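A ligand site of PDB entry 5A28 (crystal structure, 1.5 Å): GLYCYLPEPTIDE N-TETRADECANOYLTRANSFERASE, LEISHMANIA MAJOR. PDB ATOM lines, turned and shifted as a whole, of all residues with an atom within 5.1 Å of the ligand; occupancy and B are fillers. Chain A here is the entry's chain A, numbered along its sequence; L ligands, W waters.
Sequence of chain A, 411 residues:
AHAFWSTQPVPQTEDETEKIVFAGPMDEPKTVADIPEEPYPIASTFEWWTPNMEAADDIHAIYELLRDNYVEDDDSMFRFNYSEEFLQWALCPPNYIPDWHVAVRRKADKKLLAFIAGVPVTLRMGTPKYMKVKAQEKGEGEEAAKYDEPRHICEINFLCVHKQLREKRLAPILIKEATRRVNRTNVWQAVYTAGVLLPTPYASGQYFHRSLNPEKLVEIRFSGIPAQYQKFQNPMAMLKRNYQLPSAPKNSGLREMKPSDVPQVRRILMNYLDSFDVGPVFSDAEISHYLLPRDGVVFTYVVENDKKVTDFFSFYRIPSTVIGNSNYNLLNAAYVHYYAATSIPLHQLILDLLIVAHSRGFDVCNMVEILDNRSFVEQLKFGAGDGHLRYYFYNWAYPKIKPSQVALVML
Water W6 lies within hydrogen-bond range of the side-chain hydroxyl (OH) of Tyr 207 (2.8 Å) and a nitrogen (N2) of the ligand (2.9 Å).
Water W5 bridges O of Glu 72 (2.9 Å) and N3 of the ligand (3.2 Å).
Water W3 lies within hydrogen-bond range of the side-chain amide oxygen of Asn 157 (2.7 Å), the side-chain hydroxyl of Tyr 82 (2.8 Å), the chain-end carboxylate of Leu 411 (3.4 Å) and a nitrogen (N1) of the ligand (3.4 Å).
Merely in contact with the ligand: Val 71 (3.4 Å), Asp 73 (3.7 Å), Phe 78 (3.6 Å), Arg 79 (3.98 Å), Phe 80 (3.6 Å), Tyr 82 (3.1 Å), Tyr 207 (3.2 Å), Phe 208 (3.3 Å), His 209 (3.2 Å), Ile 318 (3.9 Å), Leu 331 (3.7 Å), Tyr 335 (3.7 Å), Asn 366 (3.5 Å), Met 367 (3.5 Å), Val 368 (3.96 Å) and Met 410 (3.9 Å).
Hydrophobic or aromatic side chains within 4 Å of the ligand: Val 71, Phe 78, Phe 80, Tyr 207, His 209, Ile 318, Leu 331, Tyr 335 and Val 368.
The nearest printed residue that does not touch the ligand is Phe 222 (4.02 Å).
The backbone carbonyl oxygen of Met 410 is in hydrogen-bond range of the side-chain hydroxyl of Tyr 316 (2.7 Å).
N of Leu 331 is in hydrogen-bond range of O of Ser 320.
The side-chain hydroxyl (OH) of Tyr 335 is in hydrogen-bond range of the side-chain amide nitrogen (ND2) of Asn 366 (3.2 Å).
A ring nitrogen (ND1) of His 209 lies within hydrogen-bond range of the side-chain amide oxygen (OD1) of Asn 366, 2.8 Å away.
The side-chain hydroxyl (OH) of Tyr 82 is in hydrogen-bond range of the chain-end carboxylate (OXT) of Leu 411, 2.6 Å away.
The backbone NH (N) of Phe 208 lies within hydrogen-bond range of the backbone carbonyl oxygen (O) of Met 367 (2.8 Å).
The guanidinium group (NH1) of Arg 79 is in salt-bridge range of the side-chain carboxylate (OE2) of Glu 72.
The side-chain amide nitrogen of Asn 157 sits at hydrogen-bond distance from the chain-end carboxylate of Leu 411, at 3.0 Å.
N5 of the ligand sits at hydrogen-bond distance from OG of Ser 320 (2.7 Å).
The chain-end carboxylate of Leu 411 lies within salt-bridge range of a nitrogen (N1) of the ligand (2.8 Å).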
ATOM      1  N   VAL A  71     -24.831 -17.642  17.787  1.00  0.00           N
ATOM      2  CA  VAL A  71     -24.867 -18.760  18.816  1.00  0.00           C
ATOM      3  C   VAL A  71     -23.804 -19.855  18.527  1.00  0.00           C
ATOM      4  O   VAL A  71     -23.675 -20.355  17.380  1.00  0.00           O
ATOM      5  CB  VAL A  71     -26.278 -19.429  18.898  1.00  0.00           C
ATOM      6  CG1 VAL A  71     -26.332 -20.630  19.861  1.00  0.00           C
ATOM      7  CG2 VAL A  71     -27.333 -18.373  19.416  1.00  0.00           C
ATOM      8  N   GLU A  72     -23.029 -20.220  19.569  1.00  0.00           N
ATOM      9  CA  GLU A  72     -22.138 -21.412  19.531  1.00  0.00           C
ATOM     10  C   GLU A  72     -22.631 -22.497  20.446  1.00  0.00           C
ATOM     11  O   GLU A  72     -23.458 -22.227  21.349  1.00  0.00           O
ATOM     12  CB  GLU A  72     -20.764 -20.952  20.012  1.00  0.00           C
ATOM     13  CG  GLU A  72     -20.118 -19.931  19.017  1.00  0.00           C
ATOM     14  CD  GLU A  72     -18.779 -19.358  19.492  1.00  0.00           C
ATOM     15  OE1 GLU A  72     -18.173 -19.835  20.488  1.00  0.00           O
ATOM     16  OE2 GLU A  72     -18.380 -18.342  18.862  1.00  0.00           O
ATOM     17  N   ASP A  73     -22.187 -23.732  20.199  1.00  0.00           N
ATOM     18  CA  ASP A  73     -22.437 -24.756  21.228  1.00  0.00           C
ATOM     19  C   ASP A  73     -21.603 -24.460  22.512  1.00  0.00           C
ATOM     20  O   ASP A  73     -20.795 -23.535  22.558  1.00  0.00           O
ATOM     21  CB  ASP A  73     -21.992 -26.091  20.604  1.00  0.00           C
ATOM     22  CG  ASP A  73     -20.517 -26.197  20.536  1.00  0.00           C
ATOM     23  OD1 ASP A  73     -19.920 -25.427  19.865  1.00  0.00           O
ATOM     24  OD2 ASP A  73     -19.807 -27.028  21.220  1.00  0.00           O
ATOM     25  N   PHE A  78     -18.810 -25.210  17.311  1.00  0.00           N
ATOM     26  CA  PHE A  78     -19.731 -24.919  16.201  1.00  0.00           C
ATOM     27  C   PHE A  78     -20.358 -23.554  16.417  1.00  0.00           C
ATOM     28  O   PHE A  78     -20.745 -23.219  17.549  1.00  0.00           O
ATOM     29  CB  PHE A  78     -20.865 -25.987  16.109  1.00  0.00           C
ATOM     30  CG  PHE A  78     -20.345 -27.426  16.079  1.00  0.00           C
ATOM     31  CD1 PHE A  78     -19.535 -27.905  14.996  1.00  0.00           C
ATOM     32  CD2 PHE A  78     -20.512 -28.227  17.238  1.00  0.00           C
ATOM     33  CE1 PHE A  78     -18.994 -29.210  15.058  1.00  0.00           C
ATOM     34  CE2 PHE A  78     -19.990 -29.510  17.306  1.00  0.00           C
ATOM     35  CZ  PHE A  78     -19.207 -29.959  16.207  1.00  0.00           C
ATOM     36  N   ARG A  79     -20.623 -22.854  15.300  1.00  0.00           N
ATOM     37  CA  ARG A  79     -21.366 -21.568  15.392  1.00  0.00           C
ATOM     38  C   ARG A  79     -22.389 -21.567  14.196  1.00  0.00           C
ATOM     39  O   ARG A  79     -22.010 -21.922  13.044  1.00  0.00           O
ATOM     40  CB  ARG A  79     -20.393 -20.422  15.265  1.00  0.00           C
ATOM     41  CG  ARG A  79     -21.078 -19.001  15.329  1.00  0.00           C
ATOM     42  CD  ARG A  79     -20.100 -17.857  15.741  1.00  0.00           C
ATOM     43  NE  ARG A  79     -18.970 -17.828  14.769  1.00  0.00           N
ATOM     44  CZ  ARG A  79     -17.686 -18.065  15.039  1.00  0.00           C
ATOM     45  NH1 ARG A  79     -17.202 -18.401  16.295  1.00  0.00           N
ATOM     46  NH2 ARG A  79     -16.841 -17.961  14.024  1.00  0.00           N
ATOM     47  N   PHE A  80     -23.626 -21.126  14.426  1.00  0.00           N
ATOM     48  CA  PHE A  80     -24.598 -21.082  13.335  1.00  0.00           C
ATOM     49  C   PHE A  80     -24.060 -20.232  12.206  1.00  0.00           C
ATOM     50  O   PHE A  80     -23.429 -19.135  12.453  1.00  0.00           O
ATOM     51  CB  PHE A  80     -25.948 -20.571  13.801  1.00  0.00           C
ATOM     52  CG  PHE A  80     -26.724 -21.550  14.672  1.00  0.00           C
ATOM     53  CD1 PHE A  80     -26.837 -22.886  14.324  1.00  0.00           C
ATOM     54  CD2 PHE A  80     -27.422 -21.076  15.799  1.00  0.00           C
ATOM     55  CE1 PHE A  80     -27.590 -23.739  15.132  1.00  0.00           C
ATOM     56  CE2 PHE A  80     -28.113 -21.962  16.631  1.00  0.00           C
ATOM     57  CZ  PHE A  80     -28.184 -23.299  16.297  1.00  0.00           C
ATOM     58  N   TYR A  82     -26.369 -19.107   9.468  1.00  0.00           N
ATOM     59  CA  TYR A  82     -27.547 -18.885   8.662  1.00  0.00           C
ATOM     60  C   TYR A  82     -27.252 -18.231   7.321  1.00  0.00           C
ATOM     61  O   TYR A  82     -26.416 -17.234   7.243  1.00  0.00           O
ATOM     62  CB  TYR A  82     -28.487 -17.950   9.472  1.00  0.00           C
ATOM     63  CG  TYR A  82     -29.182 -18.577  10.644  1.00  0.00           C
ATOM     64  CD1 TYR A  82     -28.585 -18.546  11.945  1.00  0.00           C
ATOM     65  CD2 TYR A  82     -30.444 -19.067  10.512  1.00  0.00           C
ATOM     66  CE1 TYR A  82     -29.301 -19.064  13.069  1.00  0.00           C
ATOM     67  CE2 TYR A  82     -31.181 -19.585  11.614  1.00  0.00           C
ATOM     68  CZ  TYR A  82     -30.621 -19.494  12.870  1.00  0.00           C
ATOM     69  OH  TYR A  82     -31.327 -19.973  13.970  1.00  0.00           O
ATOM     70  N   ASN A 157     -36.041 -12.880  17.674  1.00  0.00           N
ATOM     71  CA  ASN A 157     -34.983 -13.932  17.446  1.00  0.00           C
ATOM     72  C   ASN A 157     -33.797 -13.100  16.942  1.00  0.00           C
ATOM     73  O   ASN A 157     -33.865 -11.854  16.698  1.00  0.00           O
ATOM     74  CB  ASN A 157     -35.500 -14.890  16.351  1.00  0.00           C
ATOM     75  CG  ASN A 157     -34.804 -16.250  16.319  1.00  0.00           C
ATOM     76  OD1 ASN A 157     -33.741 -16.461  16.818  1.00  0.00           O
ATOM     77  ND2 ASN A 157     -35.469 -17.183  15.716  1.00  0.00           N
ATOM     78  N   THR A 193     -37.205 -17.622  22.459  1.00  0.00           N
ATOM     79  CA  THR A 193     -36.540 -18.723  23.114  1.00  0.00           C
ATOM     80  C   THR A 193     -35.063 -18.393  23.328  1.00  0.00           C
ATOM     81  O   THR A 193     -34.485 -17.446  22.760  1.00  0.00           O
ATOM     82  CB  THR A 193     -36.638 -20.055  22.278  1.00  0.00           C
ATOM     83  OG1 THR A 193     -36.142 -19.837  20.920  1.00  0.00           O
ATOM     84  CG2 THR A 193     -38.069 -20.639  22.255  1.00  0.00           C
ATOM     85  N   TYR A 207     -32.845 -30.867  23.646  1.00  0.00           N
ATOM     86  CA  TYR A 207     -32.462 -30.994  22.270  1.00  0.00           C
ATOM     87  C   TYR A 207     -32.331 -32.515  21.921  1.00  0.00           C
ATOM     88  O   TYR A 207     -31.943 -33.360  22.736  1.00  0.00           O
ATOM     89  CB  TYR A 207     -31.167 -30.165  22.023  1.00  0.00           C
ATOM     90  CG  TYR A 207     -31.158 -28.672  22.389  1.00  0.00           C
ATOM     91  CD1 TYR A 207     -31.801 -27.710  21.586  1.00  0.00           C
ATOM     92  CD2 TYR A 207     -30.439 -28.218  23.479  1.00  0.00           C
ATOM     93  CE1 TYR A 207     -31.714 -26.336  21.875  1.00  0.00           C
ATOM     94  CE2 TYR A 207     -30.364 -26.821  23.795  1.00  0.00           C
ATOM     95  CZ  TYR A 207     -30.989 -25.912  22.973  1.00  0.00           C
ATOM     96  OH  TYR A 207     -30.841 -24.580  23.301  1.00  0.00           O
ATOM     97  N   PHE A 208     -32.658 -32.852  20.660  1.00  0.00           N
ATOM     98  CA  PHE A 208     -32.449 -34.186  20.167  1.00  0.00           C
ATOM     99  C   PHE A 208     -31.776 -34.201  18.774  1.00  0.00           C
ATOM    100  O   PHE A 208     -32.080 -33.362  17.961  1.00  0.00           O
ATOM    101  CB  PHE A 208     -33.787 -34.979  20.079  1.00  0.00           C
ATOM    102  CG  PHE A 208     -34.315 -35.377  21.425  1.00  0.00           C
ATOM    103  CD1 PHE A 208     -35.085 -34.468  22.139  1.00  0.00           C
ATOM    104  CD2 PHE A 208     -33.993 -36.684  21.938  1.00  0.00           C
ATOM    105  CE1 PHE A 208     -35.524 -34.824  23.427  1.00  0.00           C
ATOM    106  CE2 PHE A 208     -34.482 -37.048  23.205  1.00  0.00           C
ATOM    107  CZ  PHE A 208     -35.159 -36.115  23.926  1.00  0.00           C
ATOM    108  N   HIS A 209     -30.942 -35.212  18.485  1.00  0.00           N
ATOM    109  CA  HIS A 209     -30.126 -35.289  17.232  1.00  0.00           C
ATOM    110  C   HIS A 209     -30.372 -36.668  16.665  1.00  0.00           C
ATOM    111  O   HIS A 209     -30.569 -37.599  17.406  1.00  0.00           O
ATOM    112  CB  HIS A 209     -28.623 -35.184  17.585  1.00  0.00           C
ATOM    113  CG  HIS A 209     -28.313 -33.977  18.396  1.00  0.00           C
ATOM    114  ND1 HIS A 209     -28.653 -32.724  17.956  1.00  0.00           N
ATOM    115  CD2 HIS A 209     -27.712 -33.811  19.598  1.00  0.00           C
ATOM    116  CE1 HIS A 209     -28.264 -31.819  18.855  1.00  0.00           C
ATOM    117  NE2 HIS A 209     -27.710 -32.452  19.873  1.00  0.00           N
ATOM    118  N   PHE A 222     -18.675 -33.735  16.578  1.00  0.00           N
ATOM    119  CA  PHE A 222     -20.070 -33.614  17.029  1.00  0.00           C
ATOM    120  C   PHE A 222     -20.470 -34.831  17.825  1.00  0.00           C
ATOM    121  O   PHE A 222     -21.245 -34.742  18.774  1.00  0.00           O
ATOM    122  CB  PHE A 222     -20.975 -33.551  15.803  1.00  0.00           C
ATOM    123  CG  PHE A 222     -22.414 -33.363  16.129  1.00  0.00           C
ATOM    124  CD1 PHE A 222     -22.921 -32.092  16.423  1.00  0.00           C
ATOM    125  CD2 PHE A 222     -23.256 -34.461  16.198  1.00  0.00           C
ATOM    126  CE1 PHE A 222     -24.275 -31.899  16.749  1.00  0.00           C
ATOM    127  CE2 PHE A 222     -24.603 -34.290  16.491  1.00  0.00           C
ATOM    128  CZ  PHE A 222     -25.122 -33.000  16.741  1.00  0.00           C
ATOM    129  N   TYR A 316     -36.110 -27.317   8.069  1.00  0.00           N
ATOM    130  CA  TYR A 316     -35.372 -26.177   7.558  1.00  0.00           C
ATOM    131  C   TYR A 316     -33.881 -26.421   7.752  1.00  0.00           C
ATOM    132  O   TYR A 316     -33.440 -27.210   8.544  1.00  0.00           O
ATOM    133  CB  TYR A 316     -35.856 -24.802   8.123  1.00  0.00           C
ATOM    134  CG  TYR A 316     -35.716 -24.660   9.660  1.00  0.00           C
ATOM    135  CD1 TYR A 316     -34.469 -24.396  10.250  1.00  0.00           C
ATOM    136  CD2 TYR A 316     -36.843 -24.795  10.517  1.00  0.00           C
ATOM    137  CE1 TYR A 316     -34.296 -24.223  11.645  1.00  0.00           C
ATOM    138  CE2 TYR A 316     -36.696 -24.579  11.924  1.00  0.00           C
ATOM    139  CZ  TYR A 316     -35.435 -24.330  12.444  1.00  0.00           C
ATOM    140  OH  TYR A 316     -35.247 -24.151  13.796  1.00  0.00           O
ATOM    141  N   ILE A 318     -29.970 -25.165   8.648  1.00  0.00           N
ATOM    142  CA  ILE A 318     -28.970 -24.206   9.176  1.00  0.00           C
ATOM    143  C   ILE A 318     -27.637 -24.882   9.173  1.00  0.00           C
ATOM    144  O   ILE A 318     -27.458 -25.920   9.882  1.00  0.00           O
ATOM    145  CB  ILE A 318     -29.186 -23.665  10.618  1.00  0.00           C
ATOM    146  CG1 ILE A 318     -30.669 -23.202  10.794  1.00  0.00           C
ATOM    147  CG2 ILE A 318     -28.176 -22.523  10.846  1.00  0.00           C
ATOM    148  CD1 ILE A 318     -30.968 -23.052  12.326  1.00  0.00           C
ATOM    149  N   SER A 320     -23.760 -25.147  10.298  1.00  0.00           N
ATOM    150  CA  SER A 320     -22.870 -24.577  11.320  1.00  0.00           C
ATOM    151  C   SER A 320     -21.431 -24.570  10.885  1.00  0.00           C
ATOM    152  O   SER A 320     -20.951 -25.554  10.313  1.00  0.00           O
ATOM    153  CB  SER A 320     -22.939 -25.354  12.678  1.00  0.00           C
ATOM    154  OG  SER A 320     -24.205 -25.054  13.255  1.00  0.00           O
ATOM    155  N   LEU A 331     -21.017 -28.085   9.031  1.00  0.00           N
ATOM    156  CA  LEU A 331     -21.959 -29.118   9.449  1.00  0.00           C
ATOM    157  C   LEU A 331     -23.327 -28.811   8.885  1.00  0.00           C
ATOM    158  O   LEU A 331     -23.900 -27.793   9.227  1.00  0.00           O
ATOM    159  CB  LEU A 331     -21.968 -29.218  10.963  1.00  0.00           C
ATOM    160  CG  LEU A 331     -22.992 -30.132  11.629  1.00  0.00           C
ATOM    161  CD1 LEU A 331     -22.930 -31.546  11.139  1.00  0.00           C
ATOM    162  CD2 LEU A 331     -22.487 -30.299  13.061  1.00  0.00           C
ATOM    163  N   TYR A 335     -33.440 -29.210  10.563  1.00  0.00           N
ATOM    164  CA  TYR A 335     -34.197 -29.096  11.829  1.00  0.00           C
ATOM    165  C   TYR A 335     -35.638 -29.333  11.526  1.00  0.00           C
ATOM    166  O   TYR A 335     -36.264 -28.798  10.632  1.00  0.00           O
ATOM    167  CB  TYR A 335     -34.077 -27.615  12.282  1.00  0.00           C
ATOM    168  CG  TYR A 335     -32.685 -27.316  12.758  1.00  0.00           C
ATOM    169  CD1 TYR A 335     -31.610 -27.022  11.814  1.00  0.00           C
ATOM    170  CD2 TYR A 335     -32.351 -27.295  14.135  1.00  0.00           C
ATOM    171  CE1 TYR A 335     -30.339 -26.857  12.282  1.00  0.00           C
ATOM    172  CE2 TYR A 335     -31.022 -27.124  14.575  1.00  0.00           C
ATOM    173  CZ  TYR A 335     -30.014 -26.877  13.611  1.00  0.00           C
ATOM    174  OH  TYR A 335     -28.718 -26.773  14.083  1.00  0.00           O
ATOM    175  N   ASN A 366     -31.973 -32.425  13.571  1.00  0.00           N
ATOM    176  CA  ASN A 366     -32.112 -31.925  14.910  1.00  0.00           C
ATOM    177  C   ASN A 366     -33.520 -31.468  15.236  1.00  0.00           C
ATOM    178  O   ASN A 366     -34.333 -31.104  14.314  1.00  0.00           O
ATOM    179  CB  ASN A 366     -31.233 -30.639  15.029  1.00  0.00           C
ATOM    180  CG  ASN A 366     -29.750 -30.943  15.036  1.00  0.00           C
ATOM    181  OD1 ASN A 366     -29.298 -32.028  15.354  1.00  0.00           O
ATOM    182  ND2 ASN A 366     -28.921 -29.877  14.727  1.00  0.00           N
ATOM    183  N   MET A 367     -33.914 -31.535  16.537  1.00  0.00           N
ATOM    184  CA  MET A 367     -35.242 -31.041  16.912  1.00  0.00           C
ATOM    185  C   MET A 367     -35.275 -30.838  18.437  1.00  0.00           C
ATOM    186  O   MET A 367     -34.336 -31.173  19.097  1.00  0.00           O
ATOM    187  CB  MET A 367     -36.354 -32.033  16.547  1.00  0.00           C
ATOM    188  CG  MET A 367     -36.218 -33.404  17.351  1.00  0.00           C
ATOM    189  SD  MET A 367     -37.473 -34.585  16.860  1.00  0.00           S
ATOM    190  CE  MET A 367     -37.202 -35.952  18.091  1.00  0.00           C
ATOM    191  N   VAL A 368     -36.336 -30.224  18.915  1.00  0.00           N
ATOM    192  CA  VAL A 368     -36.546 -30.035  20.361  1.00  0.00           C
ATOM    193  C   VAL A 368     -37.756 -30.956  20.664  1.00  0.00           C
ATOM    194  O   VAL A 368     -38.588 -31.229  19.826  1.00  0.00           O
ATOM    195  CB  VAL A 368     -36.912 -28.564  20.618  1.00  0.00           C
ATOM    196  CG1 VAL A 368     -37.101 -28.250  22.157  1.00  0.00           C
ATOM    197  CG2 VAL A 368     -35.831 -27.595  20.105  1.00  0.00           C
ATOM    198  N   LEU A 389     -33.736 -25.997  25.138  1.00  0.00           N
ATOM    199  CA  LEU A 389     -34.330 -24.744  24.597  1.00  0.00           C
ATOM    200  C   LEU A 389     -35.481 -24.331  25.537  1.00  0.00           C
ATOM    201  O   LEU A 389     -36.400 -25.153  25.782  1.00  0.00           O
ATOM    202  CB  LEU A 389     -34.837 -24.948  23.163  1.00  0.00           C
ATOM    203  CG  LEU A 389     -35.175 -23.583  22.583  1.00  0.00           C
ATOM    204  CD1 LEU A 389     -33.931 -22.635  22.442  1.00  0.00           C
ATOM    205  CD2 LEU A 389     -35.866 -23.759  21.260  1.00  0.00           C
ATOM    206  N   MET A 410     -39.288 -22.542  16.662  1.00  0.00           N
ATOM    207  CA  MET A 410     -38.557 -21.328  16.380  1.00  0.00           C
ATOM    208  C   MET A 410     -37.430 -21.594  15.353  1.00  0.00           C
ATOM    209  O   MET A 410     -36.886 -22.665  15.289  1.00  0.00           O
ATOM    210  CB  MET A 410     -38.014 -20.693  17.670  1.00  0.00           C
ATOM    211  CG  MET A 410     -39.121 -20.250  18.652  1.00  0.00           C
ATOM    212  SD  MET A 410     -39.208 -18.447  18.682  1.00  0.00           S
ATOM    213  CE  MET A 410     -40.239 -18.236  20.131  1.00  0.00           C
ATOM    214  N   LEU A 411     -37.128 -20.579  14.594  1.00  0.00           N
ATOM    215  CA  LEU A 411     -36.144 -20.758  13.512  1.00  0.00           C
ATOM    216  C   LEU A 411     -34.756 -20.494  14.089  1.00  0.00           C
ATOM    217  O   LEU A 411     -34.533 -20.024  15.270  1.00  0.00           O
ATOM    218  CB  LEU A 411     -36.401 -19.695  12.432  1.00  0.00           C
ATOM    219  CG  LEU A 411     -37.739 -19.849  11.722  1.00  0.00           C
ATOM    220  CD1 LEU A 411     -37.948 -18.831  10.610  1.00  0.00           C
ATOM    221  CD2 LEU A 411     -37.938 -21.260  11.179  1.00  0.00           C
ATOM    222  OXT LEU A 411     -33.779 -20.706  13.319  1.00  0.00           O
HETATM  223 CL1  LIG L   1     -31.038 -30.249  18.481  1.00  0.00          CL
HETATM  224  C1  LIG L   1     -31.252 -28.475  18.383  1.00  0.00           C
HETATM  225  C2  LIG L   1     -30.205 -27.716  18.795  1.00  0.00           C
HETATM  226  C3  LIG L   1     -32.511 -28.100  17.908  1.00  0.00           C
HETATM  227  C4  LIG L   1     -32.703 -26.645  17.871  1.00  0.00           C
HETATM  228  C5  LIG L   1     -31.645 -25.817  18.286  1.00  0.00           C
HETATM  229  O1  LIG L   1     -31.807 -24.447  18.190  1.00  0.00           O
HETATM  230  C6  LIG L   1     -32.590 -23.996  17.044  1.00  0.00           C
HETATM  231  C7  LIG L   1     -32.080 -22.898  16.028  1.00  0.00           C
HETATM  232  C8  LIG L   1     -31.946 -21.490  16.635  1.00  0.00           C
HETATM  233  N1  LIG L   1     -33.077 -21.127  17.416  1.00  0.00           N
HETATM  234  C9  LIG L   1     -33.528 -22.111  18.376  1.00  0.00           C
HETATM  235  C10 LIG L   1     -33.861 -23.433  17.656  1.00  0.00           C
HETATM  236  C11 LIG L   1     -30.465 -26.329  18.725  1.00  0.00           C
HETATM  237  C12 LIG L   1     -29.246 -25.521  19.136  1.00  0.00           C
HETATM  238  N2  LIG L   1     -29.098 -24.272  19.603  1.00  0.00           N
HETATM  239  N3  LIG L   1     -27.747 -24.145  19.811  1.00  0.00           N
HETATM  240  O2  LIG L   1     -28.026 -26.008  18.979  1.00  0.00           O
HETATM  241  C13 LIG L   1     -27.085 -25.221  19.424  1.00  0.00           C
HETATM  242  C14 LIG L   1     -25.614 -25.504  19.415  1.00  0.00           C
HETATM  243  C15 LIG L   1     -25.174 -25.847  18.008  1.00  0.00           C
HETATM  244  C16 LIG L   1     -24.642 -25.082  16.969  1.00  0.00           C
HETATM  245  C17 LIG L   1     -24.395 -23.612  16.978  1.00  0.00           C
HETATM  246  C18 LIG L   1     -25.243 -27.203  17.506  1.00  0.00           C
HETATM  247  C19 LIG L   1     -25.800 -28.467  18.190  1.00  0.00           C
HETATM  248  N4  LIG L   1     -24.806 -27.118  16.218  1.00  0.00           N
HETATM  249  N5  LIG L   1     -24.442 -25.805  15.863  1.00  0.00           N
HETATM  250  C20 LIG L   1     -24.633 -28.041  15.094  1.00  0.00           C
HETATM  251  O   HOH W   1     -35.169 -26.025  15.838  1.00  0.00           O
HETATM  252  O   HOH W   2     -36.529 -24.581  17.436  1.00  0.00           O
HETATM  253  O   HOH W   3     -31.798 -18.215  16.129  1.00  0.00           O
HETATM  254  O   HOH W   4     -31.411 -19.125  18.923  1.00  0.00           O
HETATM  255  O   HOH W   5     -26.170 -22.869  22.305  1.00  0.00           O
HETATM  256  O   HOH W   6     -30.557 -22.551  21.383  1.00  0.00           O
